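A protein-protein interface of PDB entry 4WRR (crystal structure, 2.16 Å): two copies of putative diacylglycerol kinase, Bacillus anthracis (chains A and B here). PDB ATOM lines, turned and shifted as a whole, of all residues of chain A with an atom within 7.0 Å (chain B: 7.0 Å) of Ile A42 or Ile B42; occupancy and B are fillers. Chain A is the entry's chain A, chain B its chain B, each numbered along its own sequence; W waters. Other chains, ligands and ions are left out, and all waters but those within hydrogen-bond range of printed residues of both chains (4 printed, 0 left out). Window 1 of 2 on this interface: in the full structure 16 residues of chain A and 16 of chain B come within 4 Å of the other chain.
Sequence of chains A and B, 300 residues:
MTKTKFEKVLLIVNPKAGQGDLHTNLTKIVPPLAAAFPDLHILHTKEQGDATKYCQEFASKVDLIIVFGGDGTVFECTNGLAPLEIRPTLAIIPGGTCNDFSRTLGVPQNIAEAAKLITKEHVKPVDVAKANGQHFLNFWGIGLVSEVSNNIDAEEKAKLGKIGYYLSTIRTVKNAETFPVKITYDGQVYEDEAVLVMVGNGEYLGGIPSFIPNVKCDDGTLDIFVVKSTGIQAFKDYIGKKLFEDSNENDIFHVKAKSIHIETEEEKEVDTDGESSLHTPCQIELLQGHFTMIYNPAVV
CD1 of Leu A26 touches C of Ala B34 (3.6 Å). C of Ala A34 touches CD1 of Leu B26 (3.6 Å). O of Ile B42 touches O of Pro A38, at 3.5 Å. Asp A39 touches Ile B42 (CA to O, 3.5 Å). Asp A39 touches Leu B43. Leu B40 touches His A41. O of Ile A42 touches O of Pro B38, 3.6 Å away. Ile A42 touches Asp B39 (O to CA, 3.6 Å). Ile B42 touches Ile A42 (CD1 to CD1, 3.95 Å). Leu A43 touches Asp B39 (CD2 to CG, 3.4 Å).
Water W4 lies within hydrogen-bond range of O of Pro A38 (2.6 Å) and O of His B44 (2.9 Å). Water W3 lies within hydrogen-bond range of O of Phe A37 (2.7 Å), NE2 of His B44 (3.0 Å) and O of Ile B42 (3.1 Å). Water W2 bridges O of Pro B38 (2.8 Å) and O of His A44 (3.1 Å). Water W1 lies within hydrogen-bond range of O of Phe B37, O of Ile A42 and NE2 of His A44.
N of Val A9 lies within hydrogen-bond range of O of Asp A39. The backbone carbonyl oxygen (O) of Leu A11 lies within hydrogen-bond range of the backbone NH (N) of Leu A43, 2.9 Å away. The backbone carbonyl oxygen of Leu A43 is in hydrogen-bond range of the backbone NH of Val A13, 2.9 Å away. The backbone NH of Val B9 sits at hydrogen-bond distance from the backbone carbonyl oxygen of Asp B39, 3.0 Å away. The backbone carbonyl oxygen of Val B9 is in hydrogen-bond range of the backbone NH of His B41 (2.9 Å). The backbone carbonyl oxygen (O) of His B41 is in hydrogen-bond range of the backbone NH (N) of Leu B11.
Ala A34 touches His B44, and with the chains exchanged His A44 touches Ala B34. Pro A38 touches Leu B43, and with the chains exchanged Leu A43 touches Pro B38. Leu A40 touches Ile B42, and with the chains exchanged Ile A42 touches Leu B40. Ile B42 touches its own counterpart, Ile A42.
NE2 of His B44 is in hydrogen-bond range of O of Ala A34 (2.8 Å). N of His B44 lies within hydrogen-bond range of O of Pro A38 (2.8 Å). OD1 of Asp A39 sits at hydrogen-bond distance from NE2 of His B41 (2.7 Å). The backbone carbonyl oxygen of Leu A40 is in hydrogen-bond range of the backbone NH of Ile B42, 2.8 Å away. A ring nitrogen (NE2) of His A41 is in hydrogen-bond range of the side-chain carboxylate (OD1) of Asp B39, at 2.7 Å. The backbone NH of Ile A42 lies within hydrogen-bond range of the backbone carbonyl oxygen of Leu B40 (2.8 Å). A ring nitrogen (NE2) of His A44 sits at hydrogen-bond distance from the backbone carbonyl oxygen (O) of Ala B34, at 2.8 Å. N of His A44 sits at hydrogen-bond distance from O of Pro B38 (2.9 Å).
Among the printed residues, 23 pairs touch across the chains. Among the printed residues, no Asp or Glu carboxylate lies within 4 Å of a Lys or Arg side-chain nitrogen of the other chain.
Ile A12 touches none of the printed residues of chain B. Ile A42 touches just these residues of chain B: Pro B38, Asp B39, Leu B40 and Ile B42. Of the printed residues of chain B, His A44 touches Ala B34 and Pro B38. Printed residues of chain A within 4 Å of Val B30: Val A30 (3.3 Å). Of chain A, only Pro A38 (3.5 Å), Asp A39 (3.5 Å), Leu A40 (2.8 Å) and Ile A42 (3.95 Å) come within 4 Å of Ile B42. Of the printed residues of chain A, His B44 touches Ala A34 and Pro A38. The nearest residue of chain B that does not touch Ile A42 is Ala B34 (4.5 Å). The nearest printed residue of chain A that does not touch His B44 is Phe A37 (4.1 Å).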
ATOM      1  N   VAL A   9      26.756  -2.096  -7.071  1.00  0.00           N
ATOM      2  CA  VAL A   9      27.969  -1.586  -7.636  1.00  0.00           C
ATOM      3  C   VAL A   9      28.989  -1.439  -6.552  1.00  0.00           C
ATOM      4  O   VAL A   9      28.655  -1.009  -5.449  1.00  0.00           O
ATOM      5  CB  VAL A   9      27.720  -0.233  -8.291  1.00  0.00           C
ATOM      6  CG1 VAL A   9      29.009   0.386  -8.886  1.00  0.00           C
ATOM      7  CG2 VAL A   9      26.701  -0.361  -9.377  1.00  0.00           C
ATOM      8  N   LEU A  10      30.233  -1.783  -6.862  1.00  0.00           N
ATOM      9  CA  LEU A  10      31.394  -1.497  -6.036  1.00  0.00           C
ATOM     10  C   LEU A  10      32.295  -0.510  -6.730  1.00  0.00           C
ATOM     11  O   LEU A  10      32.623  -0.688  -7.889  1.00  0.00           O
ATOM     12  CB  LEU A  10      32.193  -2.765  -5.822  1.00  0.00           C
ATOM     13  CG  LEU A  10      33.535  -2.602  -5.128  1.00  0.00           C
ATOM     14  CD1 LEU A  10      33.321  -2.255  -3.661  1.00  0.00           C
ATOM     15  CD2 LEU A  10      34.296  -3.901  -5.172  1.00  0.00           C
ATOM     16  N   LEU A  11      32.713   0.517  -6.025  1.00  0.00           N
ATOM     17  CA  LEU A  11      33.737   1.441  -6.463  1.00  0.00           C
ATOM     18  C   LEU A  11      34.984   1.274  -5.608  1.00  0.00           C
ATOM     19  O   LEU A  11      34.939   1.458  -4.371  1.00  0.00           O
ATOM     20  CB  LEU A  11      33.239   2.879  -6.325  1.00  0.00           C
ATOM     21  CG  LEU A  11      34.259   4.010  -6.513  1.00  0.00           C
ATOM     22  CD1 LEU A  11      34.775   3.992  -7.939  1.00  0.00           C
ATOM     23  CD2 LEU A  11      33.609   5.356  -6.247  1.00  0.00           C
ATOM     24  N   ILE A  12      36.087   0.888  -6.256  1.00  0.00           N
ATOM     25  CA  ILE A  12      37.388   0.754  -5.624  1.00  0.00           C
ATOM     26  C   ILE A  12      38.180   2.007  -5.862  1.00  0.00           C
ATOM     27  O   ILE A  12      38.407   2.410  -7.030  1.00  0.00           O
ATOM     28  CB  ILE A  12      38.167  -0.445  -6.184  1.00  0.00           C
ATOM     29  CG1 ILE A  12      37.411  -1.747  -5.865  1.00  0.00           C
ATOM     30  CG2 ILE A  12      39.564  -0.477  -5.594  1.00  0.00           C
ATOM     31  CD1 ILE A  12      37.967  -2.968  -6.576  1.00  0.00           C
ATOM     32  N   VAL A  13      38.589   2.665  -4.780  1.00  0.00           N
ATOM     33  CA  VAL A  13      39.292   3.928  -4.863  1.00  0.00           C
ATOM     34  C   VAL A  13      40.704   3.710  -4.425  1.00  0.00           C
ATOM     35  O   VAL A  13      40.935   3.284  -3.296  1.00  0.00           O
ATOM     36  CB  VAL A  13      38.641   4.975  -3.936  1.00  0.00           C
ATOM     37  CG1 VAL A  13      39.514   6.197  -3.825  1.00  0.00           C
ATOM     38  CG2 VAL A  13      37.275   5.376  -4.455  1.00  0.00           C
ATOM     39  N   LEU A  26      36.942  12.790  -5.191  1.00  0.00           N
ATOM     40  CA  LEU A  26      35.674  12.159  -4.819  1.00  0.00           C
ATOM     41  C   LEU A  26      34.489  13.071  -5.139  1.00  0.00           C
ATOM     42  O   LEU A  26      33.415  12.613  -5.480  1.00  0.00           O
ATOM     43  CB  LEU A  26      35.681  11.740  -3.339  1.00  0.00           C
ATOM     44  CG  LEU A  26      36.680  10.640  -3.001  1.00  0.00           C
ATOM     45  CD1 LEU A  26      36.756  10.312  -1.524  1.00  0.00           C
ATOM     46  CD2 LEU A  26      36.310   9.381  -3.738  1.00  0.00           C
ATOM     47  N   VAL A  30      32.120  10.618  -7.240  1.00  0.00           N
ATOM     48  CA  VAL A  30      31.147   9.859  -6.465  1.00  0.00           C
ATOM     49  C   VAL A  30      29.705  10.347  -6.699  1.00  0.00           C
ATOM     50  O   VAL A  30      28.817   9.541  -6.901  1.00  0.00           O
ATOM     51  CB  VAL A  30      31.511   9.831  -4.967  1.00  0.00           C
ATOM     52  CG1 VAL A  30      30.476   9.009  -4.209  1.00  0.00           C
ATOM     53  CG2 VAL A  30      32.879   9.226  -4.738  1.00  0.00           C
ATOM     54  N   ALA A  34      26.688   7.842  -7.299  1.00  0.00           N
ATOM     55  CA  ALA A  34      25.709   7.692  -6.211  1.00  0.00           C
ATOM     56  C   ALA A  34      24.311   8.123  -6.610  1.00  0.00           C
ATOM     57  O   ALA A  34      23.349   7.560  -6.108  1.00  0.00           O
ATOM     58  CB  ALA A  34      26.142   8.436  -4.976  1.00  0.00           C
ATOM     59  N   PHE A  37      23.231   5.013  -9.121  1.00  0.00           N
ATOM     60  CA  PHE A  37      23.265   3.629  -8.630  1.00  0.00           C
ATOM     61  C   PHE A  37      22.810   3.621  -7.142  1.00  0.00           C
ATOM     62  O   PHE A  37      23.564   4.033  -6.282  1.00  0.00           O
ATOM     63  CB  PHE A  37      24.680   3.068  -8.763  1.00  0.00           C
ATOM     64  CG  PHE A  37      25.169   2.977 -10.211  1.00  0.00           C
ATOM     65  CD1 PHE A  37      24.479   2.226 -11.140  1.00  0.00           C
ATOM     66  CD2 PHE A  37      26.273   3.696 -10.633  1.00  0.00           C
ATOM     67  CE1 PHE A  37      24.909   2.162 -12.470  1.00  0.00           C
ATOM     68  CE2 PHE A  37      26.715   3.618 -11.944  1.00  0.00           C
ATOM     69  CZ  PHE A  37      26.011   2.872 -12.873  1.00  0.00           C
ATOM     70  N   PRO A  38      21.557   3.215  -6.873  1.00  0.00           N
ATOM     71  CA  PRO A  38      21.002   3.281  -5.570  1.00  0.00           C
ATOM     72  C   PRO A  38      21.572   2.264  -4.558  1.00  0.00           C
ATOM     73  O   PRO A  38      21.156   2.270  -3.369  1.00  0.00           O
ATOM     74  CB  PRO A  38      19.514   3.035  -5.816  1.00  0.00           C
ATOM     75  CG  PRO A  38      19.463   2.182  -7.051  1.00  0.00           C
ATOM     76  CD  PRO A  38      20.605   2.674  -7.881  1.00  0.00           C
ATOM     77  N   ASP A  39      22.520   1.431  -4.989  1.00  0.00           N
ATOM     78  CA  ASP A  39      23.254   0.536  -4.101  1.00  0.00           C
ATOM     79  C   ASP A  39      24.719   0.560  -4.493  1.00  0.00           C
ATOM     80  O   ASP A  39      25.154  -0.214  -5.392  1.00  0.00           O
ATOM     81  CB  ASP A  39      22.644  -0.901  -4.146  1.00  0.00           C
ATOM     82  CG  ASP A  39      23.253  -1.853  -3.115  1.00  0.00           C
ATOM     83  OD1 ASP A  39      24.443  -1.687  -2.712  1.00  0.00           O
ATOM     84  OD2 ASP A  39      22.553  -2.817  -2.708  1.00  0.00           O
ATOM     85  N   LEU A  40      25.485   1.411  -3.820  1.00  0.00           N
ATOM     86  CA  LEU A  40      26.870   1.699  -4.172  1.00  0.00           C
ATOM     87  C   LEU A  40      27.787   1.536  -2.959  1.00  0.00           C
ATOM     88  O   LEU A  40      27.568   2.141  -1.915  1.00  0.00           O
ATOM     89  CB  LEU A  40      26.975   3.125  -4.716  1.00  0.00           C
ATOM     90  CG  LEU A  40      28.375   3.579  -5.091  1.00  0.00           C
ATOM     91  CD1 LEU A  40      28.956   2.790  -6.246  1.00  0.00           C
ATOM     92  CD2 LEU A  40      28.349   5.059  -5.415  1.00  0.00           C
ATOM     93  N   HIS A  41      28.821   0.699  -3.098  1.00  0.00           N
ATOM     94  CA  HIS A  41      29.722   0.423  -2.005  1.00  0.00           C
ATOM     95  C   HIS A  41      31.058   0.964  -2.459  1.00  0.00           C
ATOM     96  O   HIS A  41      31.503   0.655  -3.551  1.00  0.00           O
ATOM     97  CB  HIS A  41      29.814  -1.037  -1.770  1.00  0.00           C
ATOM     98  CG  HIS A  41      30.443  -1.407  -0.473  1.00  0.00           C
ATOM     99  ND1 HIS A  41      30.306  -2.654   0.067  1.00  0.00           N
ATOM    100  CD2 HIS A  41      31.144  -0.687   0.432  1.00  0.00           C
ATOM    101  CE1 HIS A  41      30.851  -2.685   1.274  1.00  0.00           C
ATOM    102  NE2 HIS A  41      31.396  -1.510   1.507  1.00  0.00           N
ATOM    103  N   ILE A  42      31.687   1.766  -1.613  1.00  0.00           N
ATOM    104  CA  ILE A  42      32.954   2.419  -1.898  1.00  0.00           C
ATOM    105  C   ILE A  42      34.022   1.965  -0.923  1.00  0.00           C
ATOM    106  O   ILE A  42      33.884   2.117   0.283  1.00  0.00           O
ATOM    107  CB  ILE A  42      32.793   3.949  -1.784  1.00  0.00           C
ATOM    108  CG1 ILE A  42      31.665   4.404  -2.662  1.00  0.00           C
ATOM    109  CG2 ILE A  42      34.072   4.643  -2.201  1.00  0.00           C
ATOM    110  CD1 ILE A  42      31.294   5.845  -2.434  1.00  0.00           C
ATOM    111  N   LEU A  43      35.083   1.401  -1.445  1.00  0.00           N
ATOM    112  CA  LEU A  43      36.199   0.903  -0.639  1.00  0.00           C
ATOM    113  C   LEU A  43      37.486   1.541  -1.091  1.00  0.00           C
ATOM    114  O   LEU A  43      37.817   1.463  -2.277  1.00  0.00           O
ATOM    115  CB  LEU A  43      36.380  -0.625  -0.844  1.00  0.00           C
ATOM    116  CG  LEU A  43      35.305  -1.552  -0.289  1.00  0.00           C
ATOM    117  CD1 LEU A  43      35.618  -2.974  -0.678  1.00  0.00           C
ATOM    118  CD2 LEU A  43      35.201  -1.435   1.232  1.00  0.00           C
ATOM    119  N   HIS A  44      38.261   2.070  -0.158  1.00  0.00           N
ATOM    120  CA  HIS A  44      39.583   2.565  -0.504  1.00  0.00           C
ATOM    121  C   HIS A  44      40.601   1.436  -0.361  1.00  0.00           C
ATOM    122  O   HIS A  44      40.555   0.653   0.605  1.00  0.00           O
ATOM    123  CB  HIS A  44      40.017   3.675   0.425  1.00  0.00           C
ATOM    124  CG  HIS A  44      39.076   4.834   0.485  1.00  0.00           C
ATOM    125  ND1 HIS A  44      39.411   6.012   1.119  1.00  0.00           N
ATOM    126  CD2 HIS A  44      37.808   4.988   0.053  1.00  0.00           C
ATOM    127  CE1 HIS A  44      38.402   6.856   1.036  1.00  0.00           C
ATOM    128  NE2 HIS A  44      37.438   6.278   0.347  1.00  0.00           N
ATOM    129  N   VAL B   9      30.640   1.872   7.417  1.00  0.00           N
ATOM    130  CA  VAL B   9      29.590   2.876   7.543  1.00  0.00           C
ATOM    131  C   VAL B   9      28.544   2.615   6.485  1.00  0.00           C
ATOM    132  O   VAL B   9      28.885   2.234   5.352  1.00  0.00           O
ATOM    133  CB  VAL B   9      30.175   4.265   7.371  1.00  0.00           C
ATOM    134  CG1 VAL B   9      29.109   5.361   7.401  1.00  0.00           C
ATOM    135  CG2 VAL B   9      31.208   4.506   8.420  1.00  0.00           C
ATOM    136  N   LEU B  10      27.272   2.809   6.856  1.00  0.00           N
ATOM    137  CA  LEU B  10      26.143   2.781   5.909  1.00  0.00           C
ATOM    138  C   LEU B  10      25.522   4.151   5.889  1.00  0.00           C
ATOM    139  O   LEU B  10      25.256   4.703   6.935  1.00  0.00           O
ATOM    140  CB  LEU B  10      25.078   1.807   6.367  1.00  0.00           C
ATOM    141  CG  LEU B  10      23.785   1.858   5.594  1.00  0.00           C
ATOM    142  CD1 LEU B  10      23.982   1.290   4.216  1.00  0.00           C
ATOM    143  CD2 LEU B  10      22.773   0.975   6.299  1.00  0.00           C
ATOM    144  N   LEU B  11      25.295   4.680   4.705  1.00  0.00           N
ATOM    145  CA  LEU B  11      24.540   5.880   4.489  1.00  0.00           C
ATOM    146  C   LEU B  11      23.237   5.539   3.788  1.00  0.00           C
ATOM    147  O   LEU B  11      23.247   5.000   2.652  1.00  0.00           O
ATOM    148  CB  LEU B  11      25.358   6.868   3.630  1.00  0.00           C
ATOM    149  CG  LEU B  11      24.632   8.095   3.109  1.00  0.00           C
ATOM    150  CD1 LEU B  11      24.220   8.964   4.271  1.00  0.00           C
ATOM    151  CD2 LEU B  11      25.528   8.886   2.166  1.00  0.00           C
ATOM    152  N   ILE B  12      22.131   5.824   4.455  1.00  0.00           N
ATOM    153  CA  ILE B  12      20.811   5.624   3.909  1.00  0.00           C
ATOM    154  C   ILE B  12      20.339   6.954   3.361  1.00  0.00           C
ATOM    155  O   ILE B  12      20.266   7.965   4.097  1.00  0.00           O
ATOM    156  CB  ILE B  12      19.826   5.147   4.973  1.00  0.00           C
ATOM    157  CG1 ILE B  12      20.239   3.777   5.488  1.00  0.00           C
ATOM    158  CG2 ILE B  12      18.417   5.098   4.410  1.00  0.00           C
ATOM    159  CD1 ILE B  12      19.471   3.322   6.713  1.00  0.00           C
ATOM    160  N   VAL B  13      20.001   6.976   2.067  1.00  0.00           N
ATOM    161  CA  VAL B  13      19.608   8.198   1.396  1.00  0.00           C
ATOM    162  C   VAL B  13      18.150   8.080   1.059  1.00  0.00           C
ATOM    163  O   VAL B  13      17.759   7.165   0.348  1.00  0.00           O
ATOM    164  CB  VAL B  13      20.407   8.393   0.088  1.00  0.00           C
ATOM    165  CG1 VAL B  13      19.834   9.499  -0.755  1.00  0.00           C
ATOM    166  CG2 VAL B  13      21.843   8.704   0.406  1.00  0.00           C
ATOM    167  N   LEU B  26      23.859  15.023  -3.077  1.00  0.00           N
ATOM    168  CA  LEU B  26      24.943  14.037  -2.953  1.00  0.00           C
ATOM    169  C   LEU B  26      26.306  14.665  -3.106  1.00  0.00           C
ATOM    170  O   LEU B  26      27.261  14.261  -2.472  1.00  0.00           O
ATOM    171  CB  LEU B  26      24.740  12.896  -3.931  1.00  0.00           C
ATOM    172  CG  LEU B  26      23.486  12.045  -3.659  1.00  0.00           C
ATOM    173  CD1 LEU B  26      23.248  10.982  -4.741  1.00  0.00           C
ATOM    174  CD2 LEU B  26      23.616  11.345  -2.354  1.00  0.00           C
ATOM    175  N   VAL B  30      28.208  13.377   0.195  1.00  0.00           N
ATOM    176  CA  VAL B  30      28.933  12.143   0.048  1.00  0.00           C
ATOM    177  C   VAL B  30      30.460  12.345   0.103  1.00  0.00           C
ATOM    178  O   VAL B  30      31.157  11.578   0.748  1.00  0.00           O
ATOM    179  CB  VAL B  30      28.481  11.362  -1.212  1.00  0.00           C
ATOM    180  CG1 VAL B  30      29.240  10.040  -1.319  1.00  0.00           C
ATOM    181  CG2 VAL B  30      26.988  11.037  -1.167  1.00  0.00           C
ATOM    182  N   ALA B  34      32.876   9.907   2.118  1.00  0.00           N
ATOM    183  CA  ALA B  34      33.735   9.011   1.369  1.00  0.00           C
ATOM    184  C   ALA B  34      35.212   9.296   1.549  1.00  0.00           C
ATOM    185  O   ALA B  34      35.995   8.363   1.517  1.00  0.00           O
ATOM    186  CB  ALA B  34      33.395   9.022  -0.103  1.00  0.00           C
ATOM    187  N   PHE B  37      35.762   7.951   5.416  1.00  0.00           N
ATOM    188  CA  PHE B  37      35.374   6.581   5.782  1.00  0.00           C
ATOM    189  C   PHE B  37      35.708   5.673   4.593  1.00  0.00           C
ATOM    190  O   PHE B  37      34.999   5.660   3.610  1.00  0.00           O
ATOM    191  CB  PHE B  37      33.885   6.513   6.123  1.00  0.00           C
ATOM    192  CG  PHE B  37      33.495   7.342   7.325  1.00  0.00           C
ATOM    193  CD1 PHE B  37      34.058   7.094   8.566  1.00  0.00           C
ATOM    194  CD2 PHE B  37      32.586   8.374   7.209  1.00  0.00           C
ATOM    195  CE1 PHE B  37      33.727   7.856   9.662  1.00  0.00           C
ATOM    196  CE2 PHE B  37      32.227   9.132   8.309  1.00  0.00           C
ATOM    197  CZ  PHE B  37      32.802   8.884   9.541  1.00  0.00           C
ATOM    198  N   PRO B  38      36.821   4.943   4.686  1.00  0.00           N
ATOM    199  CA  PRO B  38      37.299   4.149   3.592  1.00  0.00           C
ATOM    200  C   PRO B  38      36.470   2.863   3.295  1.00  0.00           C
ATOM    201  O   PRO B  38      36.797   2.138   2.334  1.00  0.00           O
ATOM    202  CB  PRO B  38      38.710   3.788   4.018  1.00  0.00           C
ATOM    203  CG  PRO B  38      38.655   3.722   5.515  1.00  0.00           C
ATOM    204  CD  PRO B  38      37.692   4.834   5.897  1.00  0.00           C
ATOM    205  N   ASP B  39      35.408   2.596   4.066  1.00  0.00           N
ATOM    206  CA  ASP B  39      34.443   1.560   3.747  1.00  0.00           C
ATOM    207  C   ASP B  39      33.008   2.105   3.962  1.00  0.00           C
ATOM    208  O   ASP B  39      32.482   2.094   5.109  1.00  0.00           O
ATOM    209  CB  ASP B  39      34.713   0.303   4.610  1.00  0.00           C
ATOM    210  CG  ASP B  39      33.811  -0.906   4.239  1.00  0.00           C
ATOM    211  OD1 ASP B  39      32.671  -0.719   3.740  1.00  0.00           O
ATOM    212  OD2 ASP B  39      34.242  -2.073   4.462  1.00  0.00           O
ATOM    213  N   LEU B  40      32.390   2.574   2.882  1.00  0.00           N
ATOM    214  CA  LEU B  40      31.136   3.308   2.930  1.00  0.00           C
ATOM    215  C   LEU B  40      30.122   2.724   1.924  1.00  0.00           C
ATOM    216  O   LEU B  40      30.424   2.593   0.730  1.00  0.00           O
ATOM    217  CB  LEU B  40      31.394   4.768   2.576  1.00  0.00           C
ATOM    218  CG  LEU B  40      30.161   5.665   2.527  1.00  0.00           C
ATOM    219  CD1 LEU B  40      29.498   5.813   3.889  1.00  0.00           C
ATOM    220  CD2 LEU B  40      30.525   7.027   1.997  1.00  0.00           C
ATOM    221  N   HIS B  41      28.945   2.352   2.410  1.00  0.00           N
ATOM    222  CA  HIS B  41      27.928   1.746   1.583  1.00  0.00           C
ATOM    223  C   HIS B  41      26.790   2.700   1.564  1.00  0.00           C
ATOM    224  O   HIS B  41      26.359   3.163   2.654  1.00  0.00           O
ATOM    225  CB  HIS B  41      27.504   0.447   2.194  1.00  0.00           C
ATOM    226  CG  HIS B  41      26.748  -0.436   1.273  1.00  0.00           C
ATOM    227  ND1 HIS B  41      26.543  -1.757   1.544  1.00  0.00           N
ATOM    228  CD2 HIS B  41      26.159  -0.208   0.076  1.00  0.00           C
ATOM    229  CE1 HIS B  41      25.944  -2.341   0.513  1.00  0.00           C
ATOM    230  NE2 HIS B  41      25.663  -1.417  -0.374  1.00  0.00           N
ATOM    231  N   ILE B  42      26.329   3.052   0.373  1.00  0.00           N
ATOM    232  CA  ILE B  42      25.250   3.997   0.166  1.00  0.00           C
ATOM    233  C   ILE B  42      24.023   3.298  -0.458  1.00  0.00           C
ATOM    234  O   ILE B  42      24.117   2.738  -1.540  1.00  0.00           O
ATOM    235  CB  ILE B  42      25.716   5.118  -0.745  1.00  0.00           C
ATOM    236  CG1 ILE B  42      26.985   5.720  -0.182  1.00  0.00           C
ATOM    237  CG2 ILE B  42      24.653   6.191  -0.888  1.00  0.00           C
ATOM    238  CD1 ILE B  42      27.655   6.681  -1.140  1.00  0.00           C
ATOM    239  N   LEU B  43      22.888   3.326   0.254  1.00  0.00           N
ATOM    240  CA  LEU B  43      21.651   2.747  -0.185  1.00  0.00           C
ATOM    241  C   LEU B  43      20.589   3.786  -0.250  1.00  0.00           C
ATOM    242  O   LEU B  43      20.321   4.462   0.745  1.00  0.00           O
ATOM    243  CB  LEU B  43      21.170   1.684   0.786  1.00  0.00           C
ATOM    244  CG  LEU B  43      21.960   0.408   0.891  1.00  0.00           C
ATOM    245  CD1 LEU B  43      21.382  -0.477   1.985  1.00  0.00           C
ATOM    246  CD2 LEU B  43      21.981  -0.350  -0.436  1.00  0.00           C
ATOM    247  N   HIS B  44      19.904   3.884  -1.382  1.00  0.00           N
ATOM    248  CA  HIS B  44      18.740   4.754  -1.466  1.00  0.00           C
ATOM    249  C   HIS B  44      17.484   3.991  -1.041  1.00  0.00           C
ATOM    250  O   HIS B  44      17.298   2.813  -1.386  1.00  0.00           O
ATOM    251  CB  HIS B  44      18.508   5.240  -2.891  1.00  0.00           C
ATOM    252  CG  HIS B  44      19.660   5.979  -3.503  1.00  0.00           C
ATOM    253  ND1 HIS B  44      19.537   6.667  -4.697  1.00  0.00           N
ATOM    254  CD2 HIS B  44      20.959   6.074  -3.147  1.00  0.00           C
ATOM    255  CE1 HIS B  44      20.715   7.157  -5.040  1.00  0.00           C
ATOM    256  NE2 HIS B  44      21.586   6.843  -4.099  1.00  0.00           N
HETATM  257  O   HOH W   1      34.522   5.107   0.903  1.00  0.00           O
HETATM  258  O   HOH W   2      38.356  -0.116   2.608  1.00  0.00           O
HETATM  259  O   HOH W   3      23.868   4.897  -3.701  1.00  0.00           O
HETATM  260  O   HOH W   4      19.138   0.846  -2.556  1.00  0.00           O
